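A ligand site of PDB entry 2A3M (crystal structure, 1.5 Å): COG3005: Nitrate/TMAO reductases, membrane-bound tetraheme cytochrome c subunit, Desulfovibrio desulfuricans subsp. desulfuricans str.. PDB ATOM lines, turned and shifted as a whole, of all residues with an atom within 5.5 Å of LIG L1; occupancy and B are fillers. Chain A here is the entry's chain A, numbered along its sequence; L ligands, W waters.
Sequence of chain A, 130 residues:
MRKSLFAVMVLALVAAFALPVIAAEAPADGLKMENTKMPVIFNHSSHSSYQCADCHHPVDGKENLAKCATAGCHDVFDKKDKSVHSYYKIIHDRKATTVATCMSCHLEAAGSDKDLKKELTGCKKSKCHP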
ATOM      1  N   ALA A  24      20.362 -18.315 -21.109  1.00  0.00           N
ATOM      2  CA  ALA A  24      21.703 -18.409 -20.444  1.00  0.00           C
ATOM      3  C   ALA A  24      22.797 -18.145 -21.456  1.00  0.00           C
ATOM      4  O   ALA A  24      22.573 -18.262 -22.664  1.00  0.00           O
ATOM      5  CB  ALA A  24      21.882 -19.775 -19.799  1.00  0.00           C
ATOM      6  N   GLU A  25      23.980 -17.776 -20.950  1.00  0.00           N
ATOM      7  CA  GLU A  25      25.144 -17.430 -21.779  1.00  0.00           C
ATOM      8  C   GLU A  25      26.164 -18.564 -21.833  1.00  0.00           C
ATOM      9  O   GLU A  25      26.413 -19.235 -20.830  1.00  0.00           O
ATOM     10  CB  GLU A  25      25.808 -16.171 -21.225  1.00  0.00           C
ATOM     11  CG  GLU A  25      25.134 -14.835 -21.584  1.00  0.00           C
ATOM     12  CD  GLU A  25      23.619 -14.854 -21.462  1.00  0.00           C
ATOM     13  OE1 GLU A  25      22.962 -14.994 -22.503  1.00  0.00           O
ATOM     14  OE2 GLU A  25      23.082 -14.699 -20.336  1.00  0.00           O
ATOM     15  N   ALA A  26      26.758 -18.779 -23.001  1.00  0.00           N
ATOM     16  CA  ALA A  26      27.812 -19.770 -23.149  1.00  0.00           C
ATOM     17  C   ALA A  26      29.055 -19.320 -22.364  1.00  0.00           C
ATOM     18  O   ALA A  26      29.370 -18.128 -22.324  1.00  0.00           O
ATOM     19  CB  ALA A  26      28.156 -19.968 -24.624  1.00  0.00           C
ATOM     20  N   PRO A  27      29.775 -20.282 -21.741  1.00  0.00           N
ATOM     21  CA  PRO A  27      31.001 -19.948 -21.047  1.00  0.00           C
ATOM     22  C   PRO A  27      32.181 -19.705 -21.978  1.00  0.00           C
ATOM     23  O   PRO A  27      32.092 -19.949 -23.195  1.00  0.00           O
ATOM     24  CB  PRO A  27      31.258 -21.184 -20.170  1.00  0.00           C
ATOM     25  CG  PRO A  27      30.655 -22.294 -20.929  1.00  0.00           C
ATOM     26  CD  PRO A  27      29.439 -21.714 -21.618  1.00  0.00           C
ATOM     27  N   LEU A  31      37.373 -24.885 -21.981  1.00  0.00           N
ATOM     28  CA  LEU A  31      36.769 -25.725 -20.963  1.00  0.00           C
ATOM     29  C   LEU A  31      37.375 -27.131 -21.053  1.00  0.00           C
ATOM     30  O   LEU A  31      37.478 -27.701 -22.136  1.00  0.00           O
ATOM     31  CB  LEU A  31      35.250 -25.750 -21.180  1.00  0.00           C
ATOM     32  CG  LEU A  31      34.281 -26.229 -20.117  1.00  0.00           C
ATOM     33  CD1 LEU A  31      32.890 -25.713 -20.488  1.00  0.00           C
ATOM     34  CD2 LEU A  31      34.278 -27.755 -20.011  1.00  0.00           C
ATOM     35  N   LYS A  32      37.795 -27.688 -19.909  1.00  0.00           N
ATOM     36  CA  LYS A  32      38.401 -29.018 -19.895  1.00  0.00           C
ATOM     37  C   LYS A  32      37.353 -30.090 -19.577  1.00  0.00           C
ATOM     38  O   LYS A  32      36.787 -30.098 -18.471  1.00  0.00           O
ATOM     39  CB  LYS A  32      39.545 -29.091 -18.883  1.00  0.00           C
ATOM     40  CG  LYS A  32      40.673 -28.091 -19.123  1.00  0.00           C
ATOM     41  N   MET A  33      37.092 -30.963 -20.539  1.00  0.00           N
ATOM     42  CA  MET A  33      36.322 -32.185 -20.311  1.00  0.00           C
ATOM     43  C   MET A  33      37.292 -33.249 -19.832  1.00  0.00           C
ATOM     44  O   MET A  33      38.131 -33.732 -20.608  1.00  0.00           O
ATOM     45  CB  MET A  33      35.607 -32.626 -21.594  1.00  0.00           C
ATOM     46  CG  MET A  33      34.654 -31.544 -22.137  1.00  0.00           C
ATOM     47  SD  MET A  33      33.714 -32.054 -23.590  1.00  0.00           S
ATOM     48  CE  MET A  33      32.603 -33.259 -22.907  1.00  0.00           C
ATOM     49  N   ASN A  35      36.759 -36.256 -17.417  1.00  0.00           N
ATOM     50  CA  ASN A  35      36.310 -37.418 -16.685  1.00  0.00           C
ATOM     51  C   ASN A  35      37.173 -38.639 -16.945  1.00  0.00           C
ATOM     52  O   ASN A  35      37.100 -39.633 -16.215  1.00  0.00           O
ATOM     53  CB  ASN A  35      34.852 -37.720 -17.017  1.00  0.00           C
ATOM     54  CG  ASN A  35      33.903 -36.830 -16.271  1.00  0.00           C
ATOM     55  OD1 ASN A  35      33.813 -36.900 -15.035  1.00  0.00           O
ATOM     56  ND2 ASN A  35      33.200 -35.978 -16.985  1.00  0.00           N
ATOM     57  N   PHE A  42      37.030 -28.088 -24.847  1.00  0.00           N
ATOM     58  CA  PHE A  42      35.814 -27.694 -25.529  1.00  0.00           C
ATOM     59  C   PHE A  42      35.639 -26.187 -25.590  1.00  0.00           C
ATOM     60  O   PHE A  42      35.634 -25.519 -24.555  1.00  0.00           O
ATOM     61  CB  PHE A  42      34.574 -28.347 -24.904  1.00  0.00           C
ATOM     62  CG  PHE A  42      33.305 -28.063 -25.681  1.00  0.00           C
ATOM     63  CD1 PHE A  42      33.023 -28.769 -26.850  1.00  0.00           C
ATOM     64  CD2 PHE A  42      32.425 -27.061 -25.271  1.00  0.00           C
ATOM     65  CE1 PHE A  42      31.879 -28.493 -27.589  1.00  0.00           C
ATOM     66  CE2 PHE A  42      31.278 -26.768 -25.993  1.00  0.00           C
ATOM     67  CZ  PHE A  42      30.988 -27.479 -27.164  1.00  0.00           C
ATOM     68  N   HIS A  44      33.138 -23.212 -26.705  1.00  0.00           N
ATOM     69  CA  HIS A  44      31.793 -22.835 -27.127  1.00  0.00           C
ATOM     70  C   HIS A  44      31.797 -21.940 -28.376  1.00  0.00           C
ATOM     71  O   HIS A  44      30.858 -21.989 -29.174  1.00  0.00           O
ATOM     72  CB  HIS A  44      31.009 -22.193 -25.959  1.00  0.00           C
ATOM     73  CG  HIS A  44      30.380 -23.196 -25.025  1.00  0.00           C
ATOM     74  ND1 HIS A  44      31.096 -23.833 -24.025  1.00  0.00           N
ATOM     75  CD2 HIS A  44      29.112 -23.680 -24.950  1.00  0.00           C
ATOM     76  CE1 HIS A  44      30.283 -24.659 -23.374  1.00  0.00           C
ATOM     77  NE2 HIS A  44      29.071 -24.597 -23.917  1.00  0.00           N
ATOM     78  N   HIS A  47      31.052 -23.513 -31.668  1.00  0.00           N
ATOM     79  CA  HIS A  47      29.720 -24.108 -31.735  1.00  0.00           C
ATOM     80  C   HIS A  47      28.587 -23.088 -31.536  1.00  0.00           C
ATOM     81  O   HIS A  47      27.450 -23.459 -31.303  1.00  0.00           O
ATOM     82  CB  HIS A  47      29.656 -25.224 -30.670  1.00  0.00           C
ATOM     83  CG  HIS A  47      30.672 -26.304 -30.879  1.00  0.00           C
ATOM     84  ND1 HIS A  47      31.929 -26.273 -30.305  1.00  0.00           N
ATOM     85  CD2 HIS A  47      30.637 -27.434 -31.634  1.00  0.00           C
ATOM     86  CE1 HIS A  47      32.609 -27.356 -30.675  1.00  0.00           C
ATOM     87  NE2 HIS A  47      31.856 -28.080 -31.498  1.00  0.00           N
ATOM     88  N   TYR A  50      24.918 -23.171 -33.123  1.00  0.00           N
ATOM     89  CA  TYR A  50      23.976 -24.200 -32.707  1.00  0.00           C
ATOM     90  C   TYR A  50      23.207 -23.730 -31.486  1.00  0.00           C
ATOM     91  O   TYR A  50      23.727 -22.991 -30.669  1.00  0.00           O
ATOM     92  CB  TYR A  50      24.696 -25.527 -32.409  1.00  0.00           C
ATOM     93  CG  TYR A  50      25.381 -26.053 -33.640  1.00  0.00           C
ATOM     94  CD1 TYR A  50      26.749 -25.902 -33.813  1.00  0.00           C
ATOM     95  CD2 TYR A  50      24.644 -26.645 -34.681  1.00  0.00           C
ATOM     96  CE1 TYR A  50      27.388 -26.346 -34.959  1.00  0.00           C
ATOM     97  CE2 TYR A  50      25.281 -27.098 -35.847  1.00  0.00           C
ATOM     98  CZ  TYR A  50      26.652 -26.935 -35.967  1.00  0.00           C
ATOM     99  OH  TYR A  50      27.304 -27.367 -37.099  1.00  0.00           O
ATOM    100  N   GLN A  51      21.959 -24.158 -31.382  1.00  0.00           N
ATOM    101  CA  GLN A  51      21.156 -23.837 -30.197  1.00  0.00           C
ATOM    102  C   GLN A  51      21.735 -24.552 -28.992  1.00  0.00           C
ATOM    103  O   GLN A  51      22.237 -25.672 -29.095  1.00  0.00           O
ATOM    104  CB  GLN A  51      19.714 -24.282 -30.404  1.00  0.00           C
ATOM    105  CG  GLN A  51      19.026 -23.643 -31.613  1.00  0.00           C
ATOM    106  CD  GLN A  51      18.889 -22.134 -31.507  1.00  0.00           C
ATOM    107  OE1 GLN A  51      18.488 -21.605 -30.463  1.00  0.00           O
ATOM    108  NE2 GLN A  51      19.217 -21.426 -32.581  1.00  0.00           N
ATOM    109  N   CYS A  52      21.660 -23.908 -27.815  1.00  0.00           N
ATOM    110  CA  CYS A  52      22.189 -24.524 -26.596  1.00  0.00           C
ATOM    111  C   CYS A  52      21.614 -25.923 -26.397  1.00  0.00           C
ATOM    112  O   CYS A  52      22.345 -26.836 -26.020  1.00  0.00           O
ATOM    113  CB  CYS A  52      21.893 -23.690 -25.358  1.00  0.00           C
ATOM    114  SG  CYS A  52      22.266 -21.919 -25.474  1.00  0.00           S
ATOM    115  N   ASP A  54      20.759 -28.110 -28.432  1.00  0.00           N
ATOM    116  CA  ASP A  54      21.282 -29.158 -29.329  1.00  0.00           C
ATOM    117  C   ASP A  54      22.247 -30.084 -28.586  1.00  0.00           C
ATOM    118  O   ASP A  54      22.480 -31.228 -29.016  1.00  0.00           O
ATOM    119  CB  ASP A  54      22.009 -28.568 -30.530  1.00  0.00           C
ATOM    120  CG  ASP A  54      21.074 -27.959 -31.543  1.00  0.00           C
ATOM    121  OD1 ASP A  54      21.591 -27.267 -32.443  1.00  0.00           O
ATOM    122  OD2 ASP A  54      19.842 -28.163 -31.459  1.00  0.00           O
ATOM    123  N   CYS A  55      22.821 -29.584 -27.489  1.00  0.00           N
ATOM    124  CA  CYS A  55      23.736 -30.376 -26.674  1.00  0.00           C
ATOM    125  C   CYS A  55      23.181 -30.480 -25.259  1.00  0.00           C
ATOM    126  O   CYS A  55      23.042 -31.581 -24.717  1.00  0.00           O
ATOM    127  CB  CYS A  55      25.131 -29.761 -26.663  1.00  0.00           C
ATOM    128  SG  CYS A  55      25.763 -29.593 -28.335  1.00  0.00           S
ATOM    129  N   HIS A  56      22.871 -29.328 -24.685  1.00  0.00           N
ATOM    130  CA  HIS A  56      22.267 -29.252 -23.349  1.00  0.00           C
ATOM    131  C   HIS A  56      20.764 -29.506 -23.479  1.00  0.00           C
ATOM    132  O   HIS A  56      19.947 -28.597 -23.287  1.00  0.00           O
ATOM    133  CB  HIS A  56      22.521 -27.869 -22.728  1.00  0.00           C
ATOM    134  CG  HIS A  56      23.973 -27.502 -22.610  1.00  0.00           C
ATOM    135  ND1 HIS A  56      24.815 -28.065 -21.664  1.00  0.00           N
ATOM    136  CD2 HIS A  56      24.747 -26.639 -23.328  1.00  0.00           C
ATOM    137  CE1 HIS A  56      26.031 -27.547 -21.800  1.00  0.00           C
ATOM    138  NE2 HIS A  56      26.016 -26.669 -22.801  1.00  0.00           N
ATOM    139  N   LEU A  65      21.733 -27.491 -17.836  1.00  0.00           N
ATOM    140  CA  LEU A  65      23.111 -27.109 -18.153  1.00  0.00           C
ATOM    141  C   LEU A  65      24.109 -27.911 -17.315  1.00  0.00           C
ATOM    142  O   LEU A  65      25.282 -27.530 -17.209  1.00  0.00           O
ATOM    143  CB  LEU A  65      23.341 -25.605 -17.939  1.00  0.00           C
ATOM    144  CG  LEU A  65      22.544 -24.651 -18.842  1.00  0.00           C
ATOM    145  CD1 LEU A  65      22.866 -23.202 -18.493  1.00  0.00           C
ATOM    146  CD2 LEU A  65      22.799 -24.918 -20.325  1.00  0.00           C
ATOM    147  N   ALA A  66      23.640 -29.013 -16.735  1.00  0.00           N
ATOM    148  CA  ALA A  66      24.479 -29.817 -15.827  1.00  0.00           C
ATOM    149  C   ALA A  66      25.557 -30.578 -16.583  1.00  0.00           C
ATOM    150  O   ALA A  66      25.424 -30.901 -17.766  1.00  0.00           O
ATOM    151  CB  ALA A  66      23.630 -30.775 -15.019  1.00  0.00           C
ATOM    152  N   LYS A  67      26.657 -30.881 -15.888  1.00  0.00           N
ATOM    153  CA  LYS A  67      27.729 -31.669 -16.466  1.00  0.00           C
ATOM    154  C   LYS A  67      27.219 -33.029 -16.929  1.00  0.00           C
ATOM    155  O   LYS A  67      26.449 -33.693 -16.219  1.00  0.00           O
ATOM    156  CB  LYS A  67      28.843 -31.836 -15.446  1.00  0.00           C
ATOM    157  CG  LYS A  67      29.483 -30.527 -15.000  1.00  0.00           C
ATOM    158  CD  LYS A  67      30.504 -30.060 -16.008  1.00  0.00           C
ATOM    159  CE  LYS A  67      31.720 -29.455 -15.332  1.00  0.00           C
ATOM    160  NZ  LYS A  67      32.543 -30.498 -14.651  1.00  0.00           N
ATOM    161  N   CYS A  68      27.634 -33.435 -18.124  1.00  0.00           N
ATOM    162  CA  CYS A  68      27.052 -34.609 -18.774  1.00  0.00           C
ATOM    163  C   CYS A  68      27.185 -35.902 -17.977  1.00  0.00           C
ATOM    164  O   CYS A  68      26.271 -36.726 -17.999  1.00  0.00           O
ATOM    165  CB  CYS A  68      27.650 -34.815 -20.161  1.00  0.00           C
ATOM    166  SG  CYS A  68      27.811 -33.291 -21.145  1.00  0.00           S
ATOM    167  N   ALA A  69      28.323 -36.078 -17.306  1.00  0.00           N
ATOM    168  CA  ALA A  69      28.597 -37.268 -16.510  1.00  0.00           C
ATOM    169  C   ALA A  69      28.127 -37.194 -15.046  1.00  0.00           C
ATOM    170  O   ALA A  69      28.535 -38.014 -14.223  1.00  0.00           O
ATOM    171  CB  ALA A  69      30.093 -37.620 -16.592  1.00  0.00           C
ATOM    172  N   TYR A  87      28.660 -42.650 -21.168  1.00  0.00           N
ATOM    173  CA  TYR A  87      29.389 -41.422 -21.478  1.00  0.00           C
ATOM    174  C   TYR A  87      30.122 -41.578 -22.813  1.00  0.00           C
ATOM    175  O   TYR A  87      30.182 -40.637 -23.603  1.00  0.00           O
ATOM    176  CB  TYR A  87      30.400 -41.145 -20.374  1.00  0.00           C
ATOM    177  CG  TYR A  87      31.143 -39.829 -20.479  1.00  0.00           C
ATOM    178  CD1 TYR A  87      30.496 -38.627 -20.231  1.00  0.00           C
ATOM    179  CD2 TYR A  87      32.501 -39.811 -20.770  1.00  0.00           C
ATOM    180  CE1 TYR A  87      31.197 -37.420 -20.296  1.00  0.00           C
ATOM    181  CE2 TYR A  87      33.204 -38.618 -20.810  1.00  0.00           C
ATOM    182  CZ  TYR A  87      32.534 -37.426 -20.590  1.00  0.00           C
ATOM    183  OH  TYR A  87      33.221 -36.227 -20.627  1.00  0.00           O
HETATM  184 FE1  LIG L   1      27.551 -25.651 -23.369  1.00  0.00          FE
HETATM  185  C1  LIG L   1      29.529 -26.688 -20.750  1.00  0.00           C
HETATM  186  C2  LIG L   1      26.108 -23.311 -21.375  1.00  0.00           C
HETATM  187  C3  LIG L   1      25.992 -24.290 -26.093  1.00  0.00           C
HETATM  188  C4  LIG L   1      28.371 -28.379 -25.202  1.00  0.00           C
HETATM  189  N1  LIG L   1      27.790 -25.109 -21.438  1.00  0.00           N
HETATM  190  C5  LIG L   1      28.660 -25.646 -20.520  1.00  0.00           C
HETATM  191  C6  LIG L   1      28.529 -24.912 -19.285  1.00  0.00           C
HETATM  192  C7  LIG L   1      27.585 -23.993 -19.451  1.00  0.00           C
HETATM  193  C8  LIG L   1      27.091 -24.088 -20.811  1.00  0.00           C
HETATM  194  C9  LIG L   1      27.090 -22.950 -18.422  1.00  0.00           C
HETATM  195  C10 LIG L   1      29.337 -25.164 -17.993  1.00  0.00           C
HETATM  196  C11 LIG L   1      28.710 -26.283 -17.175  1.00  0.00           C
HETATM  197  C12 LIG L   1      29.462 -26.382 -15.872  1.00  0.00           C
HETATM  198  O1  LIG L   1      28.797 -26.488 -14.804  1.00  0.00           O
HETATM  199  O2  LIG L   1      30.726 -26.346 -15.886  1.00  0.00           O
HETATM  200  N2  LIG L   1      26.307 -24.089 -23.689  1.00  0.00           N
HETATM  201  C13 LIG L   1      25.804 -23.256 -22.705  1.00  0.00           C
HETATM  202  C14 LIG L   1      24.925 -22.287 -23.326  1.00  0.00           C
HETATM  203  C15 LIG L   1      24.912 -22.556 -24.639  1.00  0.00           C
HETATM  204  C16 LIG L   1      25.770 -23.699 -24.874  1.00  0.00           C
HETATM  205  C17 LIG L   1      24.166 -21.181 -22.565  1.00  0.00           C
HETATM  206  C18 LIG L   1      24.151 -21.795 -25.749  1.00  0.00           C
HETATM  207  C19 LIG L   1      24.459 -20.488 -25.943  1.00  0.00           C
HETATM  208  N3  LIG L   1      27.242 -26.221 -25.288  1.00  0.00           N
HETATM  209  C20 LIG L   1      26.549 -25.522 -26.249  1.00  0.00           C
HETATM  210  C21 LIG L   1      26.529 -26.310 -27.465  1.00  0.00           C
HETATM  211  C22 LIG L   1      27.185 -27.442 -27.222  1.00  0.00           C
HETATM  212  C23 LIG L   1      27.634 -27.420 -25.843  1.00  0.00           C
HETATM  213  C24 LIG L   1      25.827 -25.854 -28.760  1.00  0.00           C
HETATM  214  C25 LIG L   1      27.439 -28.626 -28.194  1.00  0.00           C
HETATM  215  C26 LIG L   1      27.922 -28.485 -29.458  1.00  0.00           C
HETATM  216  N4  LIG L   1      28.758 -27.244 -23.024  1.00  0.00           N
HETATM  217  C27 LIG L   1      28.912 -28.279 -23.945  1.00  0.00           C
HETATM  218  C28 LIG L   1      29.767 -29.267 -23.373  1.00  0.00           C
HETATM  219  C29 LIG L   1      30.141 -28.767 -22.004  1.00  0.00           C
HETATM  220  C30 LIG L   1      29.469 -27.498 -21.856  1.00  0.00           C
HETATM  221  C31 LIG L   1      30.204 -30.579 -24.029  1.00  0.00           C
HETATM  222  C32 LIG L   1      31.040 -29.499 -20.990  1.00  0.00           C
HETATM  223  C33 LIG L   1      30.088 -30.363 -20.176  1.00  0.00           C
HETATM  224  C34 LIG L   1      30.873 -31.369 -19.387  1.00  0.00           C
HETATM  225  O3  LIG L   1      30.231 -32.130 -18.630  1.00  0.00           O
HETATM  226  O4  LIG L   1      32.143 -31.410 -19.481  1.00  0.00           O
HETATM  227 FE1  LG2 L   2      32.412 -29.672 -32.440  1.00  0.00          FE
HETATM  228  C1  LG2 L   2      34.692 -27.797 -34.151  1.00  0.00           C
HETATM  229  C2  LG2 L   2      34.864 -30.567 -30.183  1.00  0.00           C
HETATM  230  C3  LG2 L   2      30.096 -31.344 -30.591  1.00  0.00           C
HETATM  231  C4  LG2 L   2      30.027 -29.073 -34.838  1.00  0.00           C
HETATM  232  N1  LG2 L   2      34.385 -29.217 -32.196  1.00  0.00           N
HETATM  233  C5  LG2 L   2      35.155 -28.485 -33.061  1.00  0.00           C
HETATM  234  C6  LG2 L   2      36.539 -28.562 -32.645  1.00  0.00           C
HETATM  235  C7  LG2 L   2      36.587 -29.331 -31.556  1.00  0.00           C
HETATM  236  C8  LG2 L   2      35.229 -29.749 -31.234  1.00  0.00           C
HETATM  237  C9  LG2 L   2      37.815 -29.732 -30.726  1.00  0.00           C
HETATM  238  C10 LG2 L   2      37.724 -27.886 -33.383  1.00  0.00           C
HETATM  239  C11 LG2 L   2      37.755 -26.391 -33.068  1.00  0.00           C
HETATM  240  C12 LG2 L   2      38.073 -26.179 -31.615  1.00  0.00           C
HETATM  241  O1  LG2 L   2      39.156 -26.610 -31.162  1.00  0.00           O
HETATM  242  O2  LG2 L   2      37.229 -25.601 -30.894  1.00  0.00           O
HETATM  243  N2  LG2 L   2      32.474 -30.732 -30.705  1.00  0.00           N
HETATM  244  C13 LG2 L   2      33.590 -31.028 -29.951  1.00  0.00           C
HETATM  245  C14 LG2 L   2      33.182 -31.879 -28.844  1.00  0.00           C
HETATM  246  C15 LG2 L   2      31.849 -32.061 -28.968  1.00  0.00           C
HETATM  247  C16 LG2 L   2      31.391 -31.344 -30.138  1.00  0.00           C
HETATM  248  C17 LG2 L   2      34.131 -32.441 -27.760  1.00  0.00           C
HETATM  249  C18 LG2 L   2      30.933 -32.868 -28.054  1.00  0.00           C
HETATM  250  C19 LG2 L   2      30.971 -32.628 -26.726  1.00  0.00           C
HETATM  251  N3  LG2 L   2      30.440 -30.127 -32.685  1.00  0.00           N
HETATM  252  C20 LG2 L   2      29.668 -30.834 -31.781  1.00  0.00           C
HETATM  253  C21 LG2 L   2      28.310 -30.897 -32.256  1.00  0.00           C
HETATM  254  C22 LG2 L   2      28.285 -30.264 -33.450  1.00  0.00           C
HETATM  255  C23 LG2 L   2      29.631 -29.779 -33.736  1.00  0.00           C
HETATM  256  C24 LG2 L   2      27.169 -31.631 -31.511  1.00  0.00           C
HETATM  257  C25 LG2 L   2      27.071 -30.064 -34.384  1.00  0.00           C
HETATM  258  C26 LG2 L   2      25.803 -30.133 -33.917  1.00  0.00           C
HETATM  259  N4  LG2 L   2      32.363 -28.610 -34.183  1.00  0.00           N
HETATM  260  C27 LG2 L   2      31.275 -28.535 -35.053  1.00  0.00           C
HETATM  261  C28 LG2 L   2      31.650 -27.815 -36.242  1.00  0.00           C
HETATM  262  C29 LG2 L   2      33.120 -27.417 -36.036  1.00  0.00           C
HETATM  263  C30 LG2 L   2      33.460 -27.949 -34.733  1.00  0.00           C
HETATM  264  C31 LG2 L   2      30.753 -27.527 -37.456  1.00  0.00           C
HETATM  265  C32 LG2 L   2      34.037 -26.629 -37.000  1.00  0.00           C
HETATM  266  C33 LG2 L   2      34.079 -25.177 -36.540  1.00  0.00           C
HETATM  267  C34 LG2 L   2      35.481 -24.721 -36.198  1.00  0.00           C
HETATM  268  O3  LG2 L   2      35.630 -23.632 -35.565  1.00  0.00           O
HETATM  269  O4  LG2 L   2      36.470 -25.431 -36.540  1.00  0.00           O
HETATM  270 FE1  LG3 L   3      21.930 -36.407 -21.971  1.00  0.00          FE
HETATM  271  C1  LG3 L   3      19.953 -38.327 -23.936  1.00  0.00           C
HETATM  272  C2  LG3 L   3      24.047 -35.900 -24.642  1.00  0.00           C
HETATM  273  C3  LG3 L   3      23.607 -34.017 -20.179  1.00  0.00           C
HETATM  274  C4  LG3 L   3      20.244 -37.364 -19.170  1.00  0.00           C
HETATM  275  N1  LG3 L   3      21.964 -36.942 -23.919  1.00  0.00           N
HETATM  276  C5  LG3 L   3      21.095 -37.844 -24.486  1.00  0.00           C
HETATM  277  C6  LG3 L   3      21.566 -38.205 -25.812  1.00  0.00           C
HETATM  278  C7  LG3 L   3      22.704 -37.519 -26.024  1.00  0.00           C
HETATM  279  C8  LG3 L   3      22.968 -36.731 -24.835  1.00  0.00           C
HETATM  280  C9  LG3 L   3      23.635 -37.535 -27.247  1.00  0.00           C
HETATM  281  C10 LG3 L   3      20.836 -39.172 -26.770  1.00  0.00           C
HETATM  282  C11 LG3 L   3      20.877 -40.619 -26.281  1.00  0.00           C
HETATM  283  C12 LG3 L   3      22.267 -41.031 -25.911  1.00  0.00           C
HETATM  284  O1  LG3 L   3      23.160 -41.028 -26.803  1.00  0.00           O
HETATM  285  O2  LG3 L   3      22.483 -41.367 -24.708  1.00  0.00           O
HETATM  286  N2  LG3 L   3      23.519 -35.187 -22.332  1.00  0.00           N
HETATM  287  C13 LG3 L   3      24.246 -35.134 -23.518  1.00  0.00           C
HETATM  288  C14 LG3 L   3      25.274 -34.125 -23.349  1.00  0.00           C
HETATM  289  C15 LG3 L   3      25.141 -33.607 -22.124  1.00  0.00           C
HETATM  290  C16 LG3 L   3      24.038 -34.271 -21.455  1.00  0.00           C
HETATM  291  C17 LG3 L   3      26.310 -33.752 -24.430  1.00  0.00           C
HETATM  292  C18 LG3 L   3      25.987 -32.490 -21.492  1.00  0.00           C
HETATM  293  C19 LG3 L   3      26.227 -31.328 -22.150  1.00  0.00           C
HETATM  294  N3  LG3 L   3      21.918 -35.799 -20.042  1.00  0.00           N
HETATM  295  C20 LG3 L   3      22.690 -34.800 -19.500  1.00  0.00           C
HETATM  296  C21 LG3 L   3      22.405 -34.716 -18.087  1.00  0.00           C
HETATM  297  C22 LG3 L   3      21.474 -35.649 -17.798  1.00  0.00           C
HETATM  298  C23 LG3 L   3      21.153 -36.341 -19.029  1.00  0.00           C
HETATM  299  C24 LG3 L   3      23.079 -33.709 -17.138  1.00  0.00           C
HETATM  300  C25 LG3 L   3      20.813 -35.977 -16.431  1.00  0.00           C
HETATM  301  C26 LG3 L   3      19.966 -35.131 -15.800  1.00  0.00           C
HETATM  302  N4  LG3 L   3      20.369 -37.674 -21.612  1.00  0.00           N
HETATM  303  C27 LG3 L   3      19.790 -37.867 -20.362  1.00  0.00           C
HETATM  304  C28 LG3 L   3      18.611 -38.677 -20.532  1.00  0.00           C
HETATM  305  C29 LG3 L   3      18.513 -38.987 -22.022  1.00  0.00           C
HETATM  306  C30 LG3 L   3      19.646 -38.310 -22.605  1.00  0.00           C
HETATM  307  C31 LG3 L   3      17.640 -39.152 -19.427  1.00  0.00           C
HETATM  308  C32 LG3 L   3      17.402 -39.835 -22.693  1.00  0.00           C
HETATM  309  C33 LG3 L   3      16.671 -39.179 -23.867  1.00  0.00           C
HETATM  310  C34 LG3 L   3      16.492 -37.691 -23.730  1.00  0.00           C
HETATM  311  O3  LG3 L   3      15.996 -37.212 -22.668  1.00  0.00           O
HETATM  312  O4  LG3 L   3      16.842 -36.966 -24.700  1.00  0.00           O
HETATM  313  O   HOH W   1      33.348 -33.779 -18.982  1.00  0.00           O
HETATM  314  O   HOH W   2      26.056 -25.867 -15.148  1.00  0.00           O
HETATM  315  O   HOH W   3      25.582 -22.065 -28.834  1.00  0.00           O
HETATM  316  O   HOH W   4      27.270 -28.921 -18.956  1.00  0.00           O
HETATM  317  O   HOH W   5      30.668 -34.309 -17.199  1.00  0.00           O
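SG of Cys 52 is bonded to C18 of LIG L1, at 1.9 Å.
A ring nitrogen (NE2) of His 56 binds an iron atom (FE1) of LIG L1 (1.9 Å).
A ring nitrogen (NE2) of His 44 binds an iron atom (FE1) of LIG L1 (1.9 Å).
The side-chain sulfur of Cys 55 is bonded to a carbon (C25) of LIG L1, at 1.9 Å.
N of Cys 68 lies within hydrogen-bond range of O3 of LIG L1, at 3.0 Å.
NE2 of His 47 is bound to FE1 of LG2 L2, 1.9 Å away.
A carbon (C18) of LG3 L3 is covalently linked to the side-chain sulfur (SG) of Cys 68.
The backbone NH (N) of Phe 42 sits at hydrogen-bond distance from the backbone carbonyl oxygen (O) of Leu 31 (2.8 Å).
OD1 of Asp 54 lies within hydrogen-bond range of N of Gln 51 (3.3 Å).
Residues that only touch LIG L1: Ala 24 (3.3 Å), Glu 25 (3.4 Å), Ala 26 (3.6 Å), Pro 27 (3.4 Å), Leu 31 (3.5 Å), Met 33 (3.7 Å), Phe 42 (3.4 Å), His 47 (3.6 Å), Tyr 50 (3.8 Å), Gln 51 (3.6 Å), Leu 65 (3.6 Å) and Lys 67 (3.3 Å).
Water W1 lies within hydrogen-bond range of an oxygen (O4) of LIG L1 (2.7 Å), the side-chain hydroxyl (OH) of Tyr 87 (3.0 Å) and the side-chain amide nitrogen (ND2) of Asn 35 (3.0 Å).
Water W2 bridges O of Leu 65 (2.8 Å) and O1 of LIG L1 (2.8 Å).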
